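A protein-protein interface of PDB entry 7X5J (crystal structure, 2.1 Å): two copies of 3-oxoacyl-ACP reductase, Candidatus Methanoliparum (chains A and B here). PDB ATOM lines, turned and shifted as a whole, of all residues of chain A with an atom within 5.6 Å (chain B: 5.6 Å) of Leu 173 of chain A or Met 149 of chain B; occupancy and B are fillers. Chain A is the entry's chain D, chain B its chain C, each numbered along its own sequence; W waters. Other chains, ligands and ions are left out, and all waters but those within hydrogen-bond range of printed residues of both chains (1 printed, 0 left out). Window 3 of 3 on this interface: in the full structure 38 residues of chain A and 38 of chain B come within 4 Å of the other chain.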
ATOM      1  N   THR A 168      -4.843  -1.143   1.064  1.00  0.00           N
ATOM      2  CA  THR A 168      -5.295  -2.356   1.781  1.00  0.00           C
ATOM      3  C   THR A 168      -4.070  -3.035   2.385  1.00  0.00           C
ATOM      4  O   THR A 168      -4.118  -3.370   3.574  1.00  0.00           O
ATOM      5  CB  THR A 168      -6.099  -3.276   0.858  1.00  0.00           C
ATOM      6  OG1 THR A 168      -7.284  -2.584   0.447  1.00  0.00           O
ATOM      7  CG2 THR A 168      -6.475  -4.576   1.527  1.00  0.00           C
ATOM      8  N   LYS A 169      -3.007  -3.209   1.597  1.00  0.00           N
ATOM      9  CA  LYS A 169      -1.859  -4.065   1.990  1.00  0.00           C
ATOM     10  C   LYS A 169      -1.066  -3.382   3.118  1.00  0.00           C
ATOM     11  O   LYS A 169      -0.629  -4.114   4.051  1.00  0.00           O
ATOM     12  CB  LYS A 169      -1.043  -4.440   0.746  1.00  0.00           C
ATOM     13  CG  LYS A 169      -1.718  -5.509  -0.112  1.00  0.00           C
ATOM     14  CD  LYS A 169      -0.947  -5.951  -1.322  1.00  0.00           C
ATOM     15  CE  LYS A 169      -1.764  -6.848  -2.229  1.00  0.00           C
ATOM     16  NZ  LYS A 169      -2.094  -8.113  -1.532  1.00  0.00           N
ATOM     17  N   THR A 170      -0.866  -2.062   3.042  1.00  0.00           N
ATOM     18  CA  THR A 170      -0.153  -1.267   4.076  1.00  0.00           C
ATOM     19  C   THR A 170      -0.931  -1.349   5.398  1.00  0.00           C
ATOM     20  O   THR A 170      -0.311  -1.643   6.432  1.00  0.00           O
ATOM     21  CB  THR A 170       0.108   0.166   3.602  1.00  0.00           C
ATOM     22  OG1 THR A 170       1.313   0.139   2.828  1.00  0.00           O
ATOM     23  CG2 THR A 170       0.273   1.149   4.744  1.00  0.00           C
ATOM     24  N   VAL A 171      -2.241  -1.141   5.354  1.00  0.00           N
ATOM     25  CA  VAL A 171      -3.134  -1.108   6.554  1.00  0.00           C
ATOM     26  C   VAL A 171      -3.207  -2.513   7.150  1.00  0.00           C
ATOM     27  O   VAL A 171      -3.304  -2.620   8.381  1.00  0.00           O
ATOM     28  CB  VAL A 171      -4.549  -0.606   6.220  1.00  0.00           C
ATOM     29  CG1 VAL A 171      -5.448  -0.676   7.445  1.00  0.00           C
ATOM     30  CG2 VAL A 171      -4.538   0.806   5.669  1.00  0.00           C
ATOM     31  N   ALA A 172      -3.154  -3.552   6.312  1.00  0.00           N
ATOM     32  CA  ALA A 172      -3.076  -4.956   6.770  1.00  0.00           C
ATOM     33  C   ALA A 172      -1.788  -5.155   7.587  1.00  0.00           C
ATOM     34  O   ALA A 172      -1.859  -5.796   8.651  1.00  0.00           O
ATOM     35  CB  ALA A 172      -3.139  -5.883   5.604  1.00  0.00           C
ATOM     36  N   LEU A 173      -0.662  -4.617   7.110  1.00  0.00           N
ATOM     37  CA  LEU A 173       0.657  -4.758   7.777  1.00  0.00           C
ATOM     38  C   LEU A 173       0.634  -3.965   9.100  1.00  0.00           C
ATOM     39  O   LEU A 173       1.141  -4.458  10.086  1.00  0.00           O
ATOM     40  CB  LEU A 173       1.765  -4.264   6.839  1.00  0.00           C
ATOM     41  CG  LEU A 173       2.210  -5.208   5.716  1.00  0.00           C
ATOM     42  CD1 LEU A 173       2.962  -4.427   4.640  1.00  0.00           C
ATOM     43  CD2 LEU A 173       3.096  -6.339   6.233  1.00  0.00           C
ATOM     44  N   GLU A 174       0.039  -2.780   9.130  1.00  0.00           N
ATOM     45  CA  GLU A 174       0.041  -1.908  10.338  1.00  0.00           C
ATOM     46  C   GLU A 174      -0.984  -2.419  11.366  1.00  0.00           C
ATOM     47  O   GLU A 174      -0.749  -2.203  12.570  1.00  0.00           O
ATOM     48  CB  GLU A 174      -0.231  -0.447   9.949  1.00  0.00           C
ATOM     49  CG  GLU A 174       0.844   0.181   9.069  1.00  0.00           C
ATOM     50  CD  GLU A 174       0.575   1.626   8.673  1.00  0.00           C
ATOM     51  OE1 GLU A 174      -0.413   2.213   9.193  1.00  0.00           O
ATOM     52  OE2 GLU A 174       1.351   2.172   7.855  1.00  0.00           O
ATOM     53  N   GLY A 175      -2.048  -3.095  10.924  1.00  0.00           N
ATOM     54  CA  GLY A 175      -3.165  -3.559  11.772  1.00  0.00           C
ATOM     55  C   GLY A 175      -3.015  -4.981  12.290  1.00  0.00           C
ATOM     56  O   GLY A 175      -3.675  -5.312  13.270  1.00  0.00           O
ATOM     57  N   ALA A 176      -2.160  -5.791  11.669  1.00  0.00           N
ATOM     58  CA  ALA A 176      -2.076  -7.255  11.867  1.00  0.00           C
ATOM     59  C   ALA A 176      -1.898  -7.618  13.350  1.00  0.00           C
ATOM     60  O   ALA A 176      -2.524  -8.605  13.756  1.00  0.00           O
ATOM     61  CB  ALA A 176      -0.972  -7.834  11.015  1.00  0.00           C
ATOM     62  N   ARG A 177      -1.088  -6.883  14.123  1.00  0.00           N
ATOM     63  CA  ARG A 177      -0.731  -7.253  15.533  1.00  0.00           C
ATOM     64  C   ARG A 177      -1.897  -6.965  16.494  1.00  0.00           C
ATOM     65  O   ARG A 177      -1.831  -7.433  17.614  1.00  0.00           O
ATOM     66  CB  ARG A 177       0.529  -6.530  16.030  1.00  0.00           C
ATOM     67  CG  ARG A 177       1.815  -6.978  15.346  1.00  0.00           C
ATOM     68  CD  ARG A 177       2.995  -7.199  16.280  1.00  0.00           C
ATOM     69  NE  ARG A 177       2.880  -8.476  16.978  1.00  0.00           N
ATOM     70  CZ  ARG A 177       3.742  -8.948  17.872  1.00  0.00           C
ATOM     71  NH1 ARG A 177       4.817  -8.250  18.199  1.00  0.00           N
ATOM     72  NH2 ARG A 177       3.526 -10.126  18.430  1.00  0.00           N
ATOM     73  N   SER B 144       6.387   0.319  -7.410  1.00  0.00           N
ATOM     74  CA  SER B 144       7.233  -0.229  -6.323  1.00  0.00           C
ATOM     75  C   SER B 144       6.575  -1.493  -5.772  1.00  0.00           C
ATOM     76  O   SER B 144       5.344  -1.580  -5.770  1.00  0.00           O
ATOM     77  CB  SER B 144       7.451   0.829  -5.242  1.00  0.00           C
ATOM     78  OG  SER B 144       8.000   0.263  -4.059  1.00  0.00           O
ATOM     79  N   VAL B 145       7.378  -2.423  -5.288  1.00  0.00           N
ATOM     80  CA  VAL B 145       6.852  -3.656  -4.656  1.00  0.00           C
ATOM     81  C   VAL B 145       6.090  -3.223  -3.407  1.00  0.00           C
ATOM     82  O   VAL B 145       5.207  -3.972  -3.005  1.00  0.00           O
ATOM     83  CB  VAL B 145       7.947  -4.689  -4.345  1.00  0.00           C
ATOM     84  CG1 VAL B 145       8.587  -5.184  -5.627  1.00  0.00           C
ATOM     85  CG2 VAL B 145       9.003  -4.142  -3.384  1.00  0.00           C
ATOM     86  N   THR B 146       6.382  -2.034  -2.864  1.00  0.00           N
ATOM     87  CA  THR B 146       5.575  -1.430  -1.778  1.00  0.00           C
ATOM     88  C   THR B 146       4.115  -1.302  -2.229  1.00  0.00           C
ATOM     89  O   THR B 146       3.220  -1.559  -1.414  1.00  0.00           O
ATOM     90  CB  THR B 146       6.165  -0.093  -1.326  1.00  0.00           C
ATOM     91  OG1 THR B 146       7.437  -0.347  -0.737  1.00  0.00           O
ATOM     92  CG2 THR B 146       5.310   0.599  -0.294  1.00  0.00           C
ATOM     93  N   GLY B 147       3.886  -0.949  -3.491  1.00  0.00           N
ATOM     94  CA  GLY B 147       2.543  -0.888  -4.098  1.00  0.00           C
ATOM     95  C   GLY B 147       1.845  -2.240  -4.229  1.00  0.00           C
ATOM     96  O   GLY B 147       0.620  -2.248  -4.114  1.00  0.00           O
ATOM     97  N   THR B 148       2.563  -3.340  -4.478  1.00  0.00           N
ATOM     98  CA  THR B 148       1.963  -4.679  -4.748  1.00  0.00           C
ATOM     99  C   THR B 148       1.986  -5.562  -3.490  1.00  0.00           C
ATOM    100  O   THR B 148       1.280  -6.578  -3.472  1.00  0.00           O
ATOM    101  CB  THR B 148       2.701  -5.358  -5.912  1.00  0.00           C
ATOM    102  OG1 THR B 148       4.055  -5.466  -5.474  1.00  0.00           O
ATOM    103  CG2 THR B 148       2.656  -4.581  -7.215  1.00  0.00           C
ATOM    104  N   MET B 149       2.816  -5.238  -2.500  1.00  0.00           N
ATOM    105  CA  MET B 149       3.041  -6.087  -1.302  1.00  0.00           C
ATOM    106  C   MET B 149       2.811  -5.301  -0.014  1.00  0.00           C
ATOM    107  O   MET B 149       2.761  -5.923   1.062  1.00  0.00           O
ATOM    108  CB  MET B 149       4.464  -6.643  -1.286  1.00  0.00           C
ATOM    109  CG  MET B 149       4.704  -7.598  -2.409  1.00  0.00           C
ATOM    110  SD  MET B 149       6.312  -8.352  -2.247  1.00  0.00           S
ATOM    111  CE  MET B 149       6.078  -9.387  -0.798  1.00  0.00           C
ATOM    112  N   GLY B 150       2.627  -3.994  -0.120  1.00  0.00           N
ATOM    113  CA  GLY B 150       2.370  -3.131   1.041  1.00  0.00           C
ATOM    114  C   GLY B 150       3.672  -2.709   1.672  1.00  0.00           C
ATOM    115  O   GLY B 150       4.712  -3.318   1.386  1.00  0.00           O
ATOM    116  N   GLY B 151       3.605  -1.695   2.508  1.00  0.00           N
ATOM    117  CA  GLY B 151       4.756  -1.211   3.288  1.00  0.00           C
ATOM    118  C   GLY B 151       4.238  -0.487   4.515  1.00  0.00           C
ATOM    119  O   GLY B 151       3.474   0.513   4.363  1.00  0.00           O
ATOM    120  N   SER B 152       4.569  -1.032   5.681  1.00  0.00           N
ATOM    121  CA  SER B 152       4.235  -0.450   6.999  1.00  0.00           C
ATOM    122  C   SER B 152       4.714   0.997   7.018  1.00  0.00           C
ATOM    123  O   SER B 152       5.900   1.205   6.706  1.00  0.00           O
ATOM    124  CB  SER B 152       4.848  -1.258   8.115  1.00  0.00           C
ATOM    125  OG  SER B 152       4.279  -0.862   9.350  1.00  0.00           O
ATOM    126  N   ILE B 252      13.193  -9.514  -4.675  1.00  0.00           N
ATOM    127  CA  ILE B 252      12.691  -8.904  -3.413  1.00  0.00           C
ATOM    128  C   ILE B 252      11.238  -9.316  -3.173  1.00  0.00           C
ATOM    129  O   ILE B 252      10.800  -9.182  -2.024  1.00  0.00           O
ATOM    130  CB  ILE B 252      12.848  -7.375  -3.388  1.00  0.00           C
ATOM    131  CG1 ILE B 252      12.837  -6.866  -1.937  1.00  0.00           C
ATOM    132  CG2 ILE B 252      11.790  -6.692  -4.242  1.00  0.00           C
ATOM    133  CD1 ILE B 252      13.197  -5.404  -1.777  1.00  0.00           C
ATOM    134  N   ASP B 253      10.524  -9.748  -4.216  1.00  0.00           N
ATOM    135  CA  ASP B 253       9.060 -10.001  -4.194  1.00  0.00           C
ATOM    136  C   ASP B 253       8.792 -11.509  -4.095  1.00  0.00           C
ATOM    137  O   ASP B 253       7.627 -11.885  -4.046  1.00  0.00           O
ATOM    138  CB  ASP B 253       8.388  -9.388  -5.430  1.00  0.00           C
ATOM    139  CG  ASP B 253       8.930  -9.881  -6.764  1.00  0.00           C
ATOM    140  OD1 ASP B 253      10.172 -10.106  -6.862  1.00  0.00           O
ATOM    141  OD2 ASP B 253       8.119 -10.000  -7.714  1.00  0.00           O
HETATM  142  O   HOH W   1       0.786  -8.938  -1.542  1.00  0.00           O
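The backbone carbonyl oxygen (O) of Gly 151 of chain B sits at hydrogen-bond distance from the side-chain hydroxyl (OG1) of Thr 170 of chain A, at 2.7 Å.
O of Val 145 of chain B sits at hydrogen-bond distance from OG1 of Thr 148 of chain B (3.1 Å).
Among the printed residues, pairs that only touch across the chains: Lys 169 of chain A with Thr 148 of chain B (3.2 Å), Leu 173 of chain A with Gly 150 of chain B (3.5 Å), Leu 173 of chain A with Gly 151 of chain B (3.5 Å), Glu 174 of chain A with Ser 152 of chain B (3.6 Å), Lys 169 of chain A with Gly 150 of chain B (3.7 Å), Thr 170 of chain A with Gly 150 of chain B (3.9 Å), Leu 173 of chain A with Met 149 of chain B (3.9 Å), Leu 173 of chain A with Ser 152 of chain B (3.9 Å) and Lys 169 of chain A with Met 149 of chain B (3.99 Å).
Thr 168 of chain A touches none of the printed residues of chain B.
Of the printed residues of chain B, Thr 170 of chain A touches Gly 150 (3.9 Å) and Gly 151 (2.7 Å).
Leu 173 of chain A touches just these residues of chain B: Met 149 (3.9 Å), Gly 150 (3.5 Å), Gly 151 (3.5 Å) and Ser 152 (3.9 Å).
Of the printed residues of chain B, Glu 174 of chain A touches Ser 152.
Gly 147 of chain B touches none of the printed residues of chain A.
Printed residues of chain A within 4 Å of Met 149 of chain B: Lys 169 (3.99 Å) and Leu 173 (3.9 Å).
Of the printed residues of chain A, Gly 150 of chain B touches Lys 169, Thr 170 and Leu 173.
The nearest printed residue of chain A that does not touch Met 149 of chain B is Thr 170 of chain A (5.7 Å).
The nearest printed residue of chain A that does not touch Gly 151 of chain B is Glu 174 of chain A (4.4 Å).
Of the 11 printed residues of chain B, 5 touch a printed residue of chain A.
Among the printed residues, 10 pairs touch across the chains.
Among the printed residues, no Asp or Glu carboxylate lies within 4 Å of a Lys or Arg side-chain nitrogen of the other chain.
No position is printed for both chains.
Water W1 lies within hydrogen-bond range of NZ of Lys 169 of chain A (3.0 Å) and O of Thr 148 of chain B (3.1 Å).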
